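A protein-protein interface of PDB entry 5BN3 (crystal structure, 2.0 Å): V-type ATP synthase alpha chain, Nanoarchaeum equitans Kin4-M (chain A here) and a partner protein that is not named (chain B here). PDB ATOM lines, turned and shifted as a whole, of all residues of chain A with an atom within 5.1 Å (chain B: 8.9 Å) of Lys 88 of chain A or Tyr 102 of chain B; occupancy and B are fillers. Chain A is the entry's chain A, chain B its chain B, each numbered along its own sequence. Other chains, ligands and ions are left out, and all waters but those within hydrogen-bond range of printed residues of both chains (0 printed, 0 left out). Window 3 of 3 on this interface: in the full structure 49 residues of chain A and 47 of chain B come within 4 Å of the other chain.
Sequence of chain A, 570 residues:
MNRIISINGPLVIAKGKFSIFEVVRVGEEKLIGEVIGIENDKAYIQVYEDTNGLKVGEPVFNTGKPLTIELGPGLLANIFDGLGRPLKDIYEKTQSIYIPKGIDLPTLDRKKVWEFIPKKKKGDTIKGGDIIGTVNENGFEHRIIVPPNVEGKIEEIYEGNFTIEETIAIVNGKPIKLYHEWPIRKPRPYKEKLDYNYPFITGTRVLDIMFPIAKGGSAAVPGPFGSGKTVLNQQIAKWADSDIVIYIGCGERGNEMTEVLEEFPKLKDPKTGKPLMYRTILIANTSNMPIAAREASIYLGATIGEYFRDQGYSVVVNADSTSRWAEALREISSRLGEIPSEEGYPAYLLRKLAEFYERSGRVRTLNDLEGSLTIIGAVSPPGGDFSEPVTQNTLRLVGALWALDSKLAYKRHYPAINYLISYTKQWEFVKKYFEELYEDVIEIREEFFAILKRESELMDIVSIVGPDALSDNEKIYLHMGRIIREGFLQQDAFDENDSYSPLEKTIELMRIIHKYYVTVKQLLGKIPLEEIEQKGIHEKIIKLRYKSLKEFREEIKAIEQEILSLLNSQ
Among the printed residues, merely in contact across the chains: Leu 87 of chain A with Pro 101 of chain B (3.6 Å), Lys 88 of chain A with Tyr 102 of chain B (3.5 Å), Tyr 91 of chain A with Asn 100 of chain B (3.9 Å), Tyr 91 of chain A with Tyr 102 of chain B (3.8 Å), Tyr 91 of chain A with Ala 103 of chain B (3.8 Å), Thr 258 of chain A with Arg 104 of chain B (3.3 Å) and Thr 258 of chain A with Val 106 of chain B (3.9 Å).
Of the printed residues of chain B, Leu 87 of chain A touches Asn 100 and Pro 101.
Of chain B, only Tyr 102 (3.5 Å) comes within 4 Å of Lys 88 of chain A.
Printed residues of chain A within 4 Å of Asn 100 of chain B: Leu 87 (2.9 Å) and Tyr 91 (3.9 Å).
Tyr 102 of chain B touches just these residues of chain A: Lys 88 and Tyr 91.
Of the printed residues of chain A, Arg 104 of chain B touches Thr 258 (3.3 Å).
The nearest residue of chain B that does not touch Lys 88 of chain A is Asn 100 of chain B (5.0 Å).
The nearest printed residue of chain B that does not touch Tyr 91 of chain A is Ser 270 of chain B (6.0 Å).
The side-chain amino group of Lys 88 of chain A lies within salt-bridge range of the side-chain carboxylate of Glu 92 of chain A, at 3.0 Å.
O of Ile 79 of chain A lies within hydrogen-bond range of N of Leu 87 of chain A (3.1 Å).
OD1 of Asn 100 of chain B sits at hydrogen-bond distance from N of Tyr 102 of chain B (3.0 Å).
The side-chain hydroxyl (OG1) of Thr 269 of chain B lies within hydrogen-bond range of the backbone carbonyl oxygen (O) of Ala 103 of chain B.
The side-chain hydroxyl of Thr 258 of chain A is in hydrogen-bond range of the backbone carbonyl oxygen of Pro 101 of chain B (2.7 Å).
The backbone carbonyl oxygen of Leu 87 of chain A is in hydrogen-bond range of the side-chain amide nitrogen of Asn 100 of chain B.
Hydrophobic or aromatic side chains of chain B within 4 Å of the printed part of chain A: Pro 101, Tyr 102, Ala 103 and Val 106.
Hydrophobic or aromatic side chains of chain A that line the printed part of chain B: Leu 87 and Tyr 91.
Along chain A the printed residues that touch a printed residue of chain B span positions 87 to 258.
Among the printed residues, 9 pairs touch across the chains.
Among the printed residues, no Asp or Glu carboxylate lies within 4 Å of a Lys or Arg side-chain nitrogen of the other chain.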
ATOM      1  N   ASN A  78      16.044 -40.380   1.636  1.00  0.00           N
ATOM      2  CA  ASN A  78      16.159 -38.985   1.217  1.00  0.00           C
ATOM      3  C   ASN A  78      14.812 -38.342   0.898  1.00  0.00           C
ATOM      4  O   ASN A  78      13.821 -39.036   0.660  1.00  0.00           O
ATOM      5  CB  ASN A  78      17.109 -38.861   0.023  1.00  0.00           C
ATOM      6  CG  ASN A  78      18.565 -38.970   0.427  1.00  0.00           C
ATOM      7  OD1 ASN A  78      19.030 -38.245   1.309  1.00  0.00           O
ATOM      8  ND2 ASN A  78      19.290 -39.886  -0.203  1.00  0.00           N
ATOM      9  N   ILE A  79      14.786 -37.012   0.898  1.00  0.00           N
ATOM     10  CA  ILE A  79      13.571 -36.264   0.588  1.00  0.00           C
ATOM     11  C   ILE A  79      13.741 -35.439  -0.689  1.00  0.00           C
ATOM     12  O   ILE A  79      14.752 -34.757  -0.875  1.00  0.00           O
ATOM     13  CB  ILE A  79      13.130 -35.377   1.779  1.00  0.00           C
ATOM     14  CG1 ILE A  79      11.862 -34.589   1.438  1.00  0.00           C
ATOM     15  CG2 ILE A  79      14.255 -34.447   2.217  1.00  0.00           C
ATOM     16  CD1 ILE A  79      11.275 -33.840   2.624  1.00  0.00           C
ATOM     17  N   PRO A  86      16.531 -32.997  -4.915  1.00  0.00           N
ATOM     18  CA  PRO A  86      16.847 -33.290  -3.511  1.00  0.00           C
ATOM     19  C   PRO A  86      16.866 -32.029  -2.655  1.00  0.00           C
ATOM     20  O   PRO A  86      17.654 -31.118  -2.916  1.00  0.00           O
ATOM     21  CB  PRO A  86      18.251 -33.900  -3.591  1.00  0.00           C
ATOM     22  CG  PRO A  86      18.847 -33.316  -4.831  1.00  0.00           C
ATOM     23  CD  PRO A  86      17.706 -33.137  -5.795  1.00  0.00           C
ATOM     24  N   LEU A  87      16.013 -31.990  -1.634  1.00  0.00           N
ATOM     25  CA  LEU A  87      15.854 -30.799  -0.806  1.00  0.00           C
ATOM     26  C   LEU A  87      17.048 -30.543   0.113  1.00  0.00           C
ATOM     27  O   LEU A  87      17.302 -29.403   0.506  1.00  0.00           O
ATOM     28  CB  LEU A  87      14.562 -30.892   0.008  1.00  0.00           C
ATOM     29  CG  LEU A  87      13.276 -30.848  -0.822  1.00  0.00           C
ATOM     30  CD1 LEU A  87      12.049 -31.004   0.055  1.00  0.00           C
ATOM     31  CD2 LEU A  87      13.211 -29.544  -1.587  1.00  0.00           C
ATOM     32  N   LYS A  88      17.769 -31.603   0.461  1.00  0.00           N
ATOM     33  CA  LYS A  88      18.963 -31.477   1.291  1.00  0.00           C
ATOM     34  C   LYS A  88      20.052 -30.747   0.517  1.00  0.00           C
ATOM     35  O   LYS A  88      20.718 -29.858   1.052  1.00  0.00           O
ATOM     36  CB  LYS A  88      19.455 -32.859   1.731  1.00  0.00           C
ATOM     37  CG  LYS A  88      20.767 -32.847   2.505  1.00  0.00           C
ATOM     38  CD  LYS A  88      21.111 -34.237   3.033  1.00  0.00           C
ATOM     39  CE  LYS A  88      22.485 -34.263   3.685  1.00  0.00           C
ATOM     40  NZ  LYS A  88      23.577 -34.029   2.703  1.00  0.00           N
ATOM     41  N   ASP A  89      20.218 -31.116  -0.751  1.00  0.00           N
ATOM     42  CA  ASP A  89      21.217 -30.487  -1.612  1.00  0.00           C
ATOM     43  C   ASP A  89      20.854 -29.039  -1.946  1.00  0.00           C
ATOM     44  O   ASP A  89      21.733 -28.185  -2.038  1.00  0.00           O
ATOM     45  CB  ASP A  89      21.421 -31.302  -2.896  1.00  0.00           C
ATOM     46  CG  ASP A  89      21.992 -32.686  -2.628  1.00  0.00           C
ATOM     47  OD1 ASP A  89      22.396 -32.956  -1.477  1.00  0.00           O
ATOM     48  OD2 ASP A  89      22.045 -33.498  -3.575  1.00  0.00           O
ATOM     49  N   ILE A  90      19.563 -28.769  -2.130  1.00  0.00           N
ATOM     50  CA  ILE A  90      19.088 -27.406  -2.359  1.00  0.00           C
ATOM     51  C   ILE A  90      19.447 -26.527  -1.166  1.00  0.00           C
ATOM     52  O   ILE A  90      19.948 -25.414  -1.331  1.00  0.00           O
ATOM     53  CB  ILE A  90      17.558 -27.363  -2.582  1.00  0.00           C
ATOM     54  CG1 ILE A  90      17.185 -28.052  -3.897  1.00  0.00           C
ATOM     55  CG2 ILE A  90      17.054 -25.933  -2.589  1.00  0.00           C
ATOM     56  CD1 ILE A  90      15.690 -28.092  -4.163  1.00  0.00           C
ATOM     57  N   TYR A  91      19.200 -27.041   0.036  1.00  0.00           N
ATOM     58  CA  TYR A  91      19.548 -26.331   1.260  1.00  0.00           C
ATOM     59  C   TYR A  91      21.043 -26.033   1.323  1.00  0.00           C
ATOM     60  O   TYR A  91      21.446 -24.920   1.652  1.00  0.00           O
ATOM     61  CB  TYR A  91      19.135 -27.148   2.488  1.00  0.00           C
ATOM     62  CG  TYR A  91      19.589 -26.550   3.802  1.00  0.00           C
ATOM     63  CD1 TYR A  91      18.870 -25.530   4.405  1.00  0.00           C
ATOM     64  CD2 TYR A  91      20.733 -27.009   4.440  1.00  0.00           C
ATOM     65  CE1 TYR A  91      19.279 -24.979   5.605  1.00  0.00           C
ATOM     66  CE2 TYR A  91      21.150 -26.463   5.642  1.00  0.00           C
ATOM     67  CZ  TYR A  91      20.417 -25.449   6.218  1.00  0.00           C
ATOM     68  OH  TYR A  91      20.824 -24.903   7.411  1.00  0.00           O
ATOM     69  N   GLU A  92      21.860 -27.034   1.009  1.00  0.00           N
ATOM     70  CA  GLU A  92      23.311 -26.901   1.118  1.00  0.00           C
ATOM     71  C   GLU A  92      23.919 -25.964   0.072  1.00  0.00           C
ATOM     72  O   GLU A  92      24.830 -25.197   0.384  1.00  0.00           O
ATOM     73  CB  GLU A  92      23.983 -28.280   1.090  1.00  0.00           C
ATOM     74  CG  GLU A  92      23.891 -29.026   2.420  1.00  0.00           C
ATOM     75  CD  GLU A  92      24.271 -30.492   2.318  1.00  0.00           C
ATOM     76  OE1 GLU A  92      24.639 -30.945   1.212  1.00  0.00           O
ATOM     77  OE2 GLU A  92      24.194 -31.196   3.347  1.00  0.00           O
ATOM     78  N   THR A 258       8.634 -32.565   7.586  1.00  0.00           N
ATOM     79  CA  THR A 258       9.694 -32.369   8.572  1.00  0.00           C
ATOM     80  C   THR A 258       9.547 -33.336   9.748  1.00  0.00           C
ATOM     81  O   THR A 258      10.539 -33.841  10.275  1.00  0.00           O
ATOM     82  CB  THR A 258       9.692 -30.921   9.101  1.00  0.00           C
ATOM     83  OG1 THR A 258       9.634 -30.005   7.998  1.00  0.00           O
ATOM     84  CG2 THR A 258      10.939 -30.650   9.919  1.00  0.00           C
ATOM     85  N   LEU A 261      10.988 -36.613   8.808  1.00  0.00           N
ATOM     86  CA  LEU A 261      12.442 -36.469   8.818  1.00  0.00           C
ATOM     87  C   LEU A 261      13.013 -36.534  10.232  1.00  0.00           C
ATOM     88  O   LEU A 261      14.114 -37.042  10.439  1.00  0.00           O
ATOM     89  CB  LEU A 261      12.854 -35.147   8.165  1.00  0.00           C
ATOM     90  CG  LEU A 261      12.694 -35.009   6.652  1.00  0.00           C
ATOM     91  CD1 LEU A 261      13.091 -33.610   6.197  1.00  0.00           C
ATOM     92  CD2 LEU A 261      13.534 -36.050   5.945  1.00  0.00           C
ATOM     93  N   ILE B  99       9.316 -22.132   2.170  1.00  0.00           N
ATOM     94  CA  ILE B  99      10.352 -22.639   3.064  1.00  0.00           C
ATOM     95  C   ILE B  99      10.647 -24.107   2.749  1.00  0.00           C
ATOM     96  O   ILE B  99       9.733 -24.901   2.523  1.00  0.00           O
ATOM     97  CB  ILE B  99       9.936 -22.485   4.547  1.00  0.00           C
ATOM     98  CG1 ILE B  99       9.789 -21.003   4.908  1.00  0.00           C
ATOM     99  CG2 ILE B  99      10.952 -23.135   5.468  1.00  0.00           C
ATOM    100  CD1 ILE B  99       9.280 -20.761   6.322  1.00  0.00           C
ATOM    101  N   ASN B 100      11.929 -24.456   2.715  1.00  0.00           N
ATOM    102  CA  ASN B 100      12.351 -25.837   2.531  1.00  0.00           C
ATOM    103  C   ASN B 100      12.026 -26.647   3.788  1.00  0.00           C
ATOM    104  O   ASN B 100      12.525 -26.334   4.868  1.00  0.00           O
ATOM    105  CB  ASN B 100      13.858 -25.863   2.268  1.00  0.00           C
ATOM    106  CG  ASN B 100      14.350 -27.203   1.762  1.00  0.00           C
ATOM    107  OD1 ASN B 100      13.746 -28.246   2.020  1.00  0.00           O
ATOM    108  ND2 ASN B 100      15.468 -27.180   1.046  1.00  0.00           N
ATOM    109  N   PRO B 101      11.189 -27.691   3.652  1.00  0.00           N
ATOM    110  CA  PRO B 101      10.818 -28.513   4.814  1.00  0.00           C
ATOM    111  C   PRO B 101      12.017 -29.210   5.455  1.00  0.00           C
ATOM    112  O   PRO B 101      11.941 -29.588   6.624  1.00  0.00           O
ATOM    113  CB  PRO B 101       9.839 -29.544   4.229  1.00  0.00           C
ATOM    114  CG  PRO B 101      10.091 -29.535   2.754  1.00  0.00           C
ATOM    115  CD  PRO B 101      10.512 -28.135   2.422  1.00  0.00           C
ATOM    116  N   TYR B 102      13.103 -29.377   4.703  1.00  0.00           N
ATOM    117  CA  TYR B 102      14.347 -29.901   5.261  1.00  0.00           C
ATOM    118  C   TYR B 102      14.931 -28.908   6.260  1.00  0.00           C
ATOM    119  O   TYR B 102      15.602 -29.295   7.216  1.00  0.00           O
ATOM    120  CB  TYR B 102      15.365 -30.181   4.147  1.00  0.00           C
ATOM    121  CG  TYR B 102      16.701 -30.709   4.634  1.00  0.00           C
ATOM    122  CD1 TYR B 102      16.856 -32.043   4.987  1.00  0.00           C
ATOM    123  CD2 TYR B 102      17.811 -29.878   4.727  1.00  0.00           C
ATOM    124  CE1 TYR B 102      18.076 -32.532   5.430  1.00  0.00           C
ATOM    125  CE2 TYR B 102      19.033 -30.359   5.169  1.00  0.00           C
ATOM    126  CZ  TYR B 102      19.159 -31.685   5.518  1.00  0.00           C
ATOM    127  OH  TYR B 102      20.371 -32.165   5.955  1.00  0.00           O
ATOM    128  N   ALA B 103      14.664 -27.626   6.034  1.00  0.00           N
ATOM    129  CA  ALA B 103      15.211 -26.563   6.872  1.00  0.00           C
ATOM    130  C   ALA B 103      14.351 -26.266   8.099  1.00  0.00           C
ATOM    131  O   ALA B 103      14.782 -25.548   9.001  1.00  0.00           O
ATOM    132  CB  ALA B 103      15.405 -25.303   6.057  1.00  0.00           C
ATOM    133  N   ARG B 104      13.138 -26.809   8.129  1.00  0.00           N
ATOM    134  CA  ARG B 104      12.224 -26.569   9.243  1.00  0.00           C
ATOM    135  C   ARG B 104      12.588 -27.355  10.496  1.00  0.00           C
ATOM    136  O   ARG B 104      13.287 -28.368  10.435  1.00  0.00           O
ATOM    137  CB  ARG B 104      10.788 -26.936   8.856  1.00  0.00           C
ATOM    138  CG  ARG B 104      10.099 -25.966   7.914  1.00  0.00           C
ATOM    139  CD  ARG B 104       8.655 -26.398   7.673  1.00  0.00           C
ATOM    140  NE  ARG B 104       7.942 -25.498   6.771  1.00  0.00           N
ATOM    141  CZ  ARG B 104       7.313 -24.396   7.166  1.00  0.00           C
ATOM    142  NH1 ARG B 104       7.314 -24.061   8.449  1.00  0.00           N
ATOM    143  NH2 ARG B 104       6.689 -23.629   6.285  1.00  0.00           N
ATOM    144  N   LYS B 105      12.098 -26.865  11.630  1.00  0.00           N
ATOM    145  CA  LYS B 105      12.058 -27.637  12.864  1.00  0.00           C
ATOM    146  C   LYS B 105      10.602 -27.709  13.311  1.00  0.00           C
ATOM    147  O   LYS B 105       9.892 -26.702  13.277  1.00  0.00           O
ATOM    148  CB  LYS B 105      12.903 -26.970  13.950  1.00  0.00           C
ATOM    149  CG  LYS B 105      12.773 -27.626  15.318  1.00  0.00           C
ATOM    150  CD  LYS B 105      13.561 -26.858  16.369  1.00  0.00           C
ATOM    151  CE  LYS B 105      13.204 -27.319  17.774  1.00  0.00           C
ATOM    152  NZ  LYS B 105      13.821 -26.446  18.812  1.00  0.00           N
ATOM    153  N   VAL B 106      10.150 -28.892  13.713  1.00  0.00           N
ATOM    154  CA  VAL B 106       8.775 -29.055  14.174  1.00  0.00           C
ATOM    155  C   VAL B 106       8.588 -28.382  15.532  1.00  0.00           C
ATOM    156  O   VAL B 106       9.345 -28.651  16.463  1.00  0.00           O
ATOM    157  CB  VAL B 106       8.388 -30.542  14.279  1.00  0.00           C
ATOM    158  CG1 VAL B 106       6.955 -30.685  14.759  1.00  0.00           C
ATOM    159  CG2 VAL B 106       8.564 -31.228  12.932  1.00  0.00           C
ATOM    160  N   LEU B 268       8.924 -22.703  12.550  1.00  0.00           N
ATOM    161  CA  LEU B 268      10.073 -22.662  13.435  1.00  0.00           C
ATOM    162  C   LEU B 268      11.328 -23.106  12.699  1.00  0.00           C
ATOM    163  O   LEU B 268      11.299 -24.052  11.909  1.00  0.00           O
ATOM    164  CB  LEU B 268       9.823 -23.563  14.646  1.00  0.00           C
ATOM    165  CG  LEU B 268      10.940 -23.730  15.675  1.00  0.00           C
ATOM    166  CD1 LEU B 268      11.177 -22.428  16.402  1.00  0.00           C
ATOM    167  CD2 LEU B 268      10.582 -24.830  16.661  1.00  0.00           C
ATOM    168  N   THR B 269      12.424 -22.403  12.958  1.00  0.00           N
ATOM    169  CA  THR B 269      13.726 -22.768  12.418  1.00  0.00           C
ATOM    170  C   THR B 269      14.728 -22.652  13.564  1.00  0.00           C
ATOM    171  O   THR B 269      14.350 -22.279  14.674  1.00  0.00           O
ATOM    172  CB  THR B 269      14.115 -21.860  11.229  1.00  0.00           C
ATOM    173  OG1 THR B 269      15.110 -22.503  10.423  1.00  0.00           O
ATOM    174  CG2 THR B 269      14.643 -20.521  11.718  1.00  0.00           C
ATOM    175  N   SER B 270      15.993 -22.977  13.317  1.00  0.00           N
ATOM    176  CA  SER B 270      17.000 -22.881  14.368  1.00  0.00           C
ATOM    177  C   SER B 270      17.254 -21.434  14.794  1.00  0.00           C
ATOM    178  O   SER B 270      17.671 -21.175  15.924  1.00  0.00           O
ATOM    179  CB  SER B 270      18.309 -23.543  13.928  1.00  0.00           C
ATOM    180  OG  SER B 270      18.803 -22.951  12.741  1.00  0.00           O
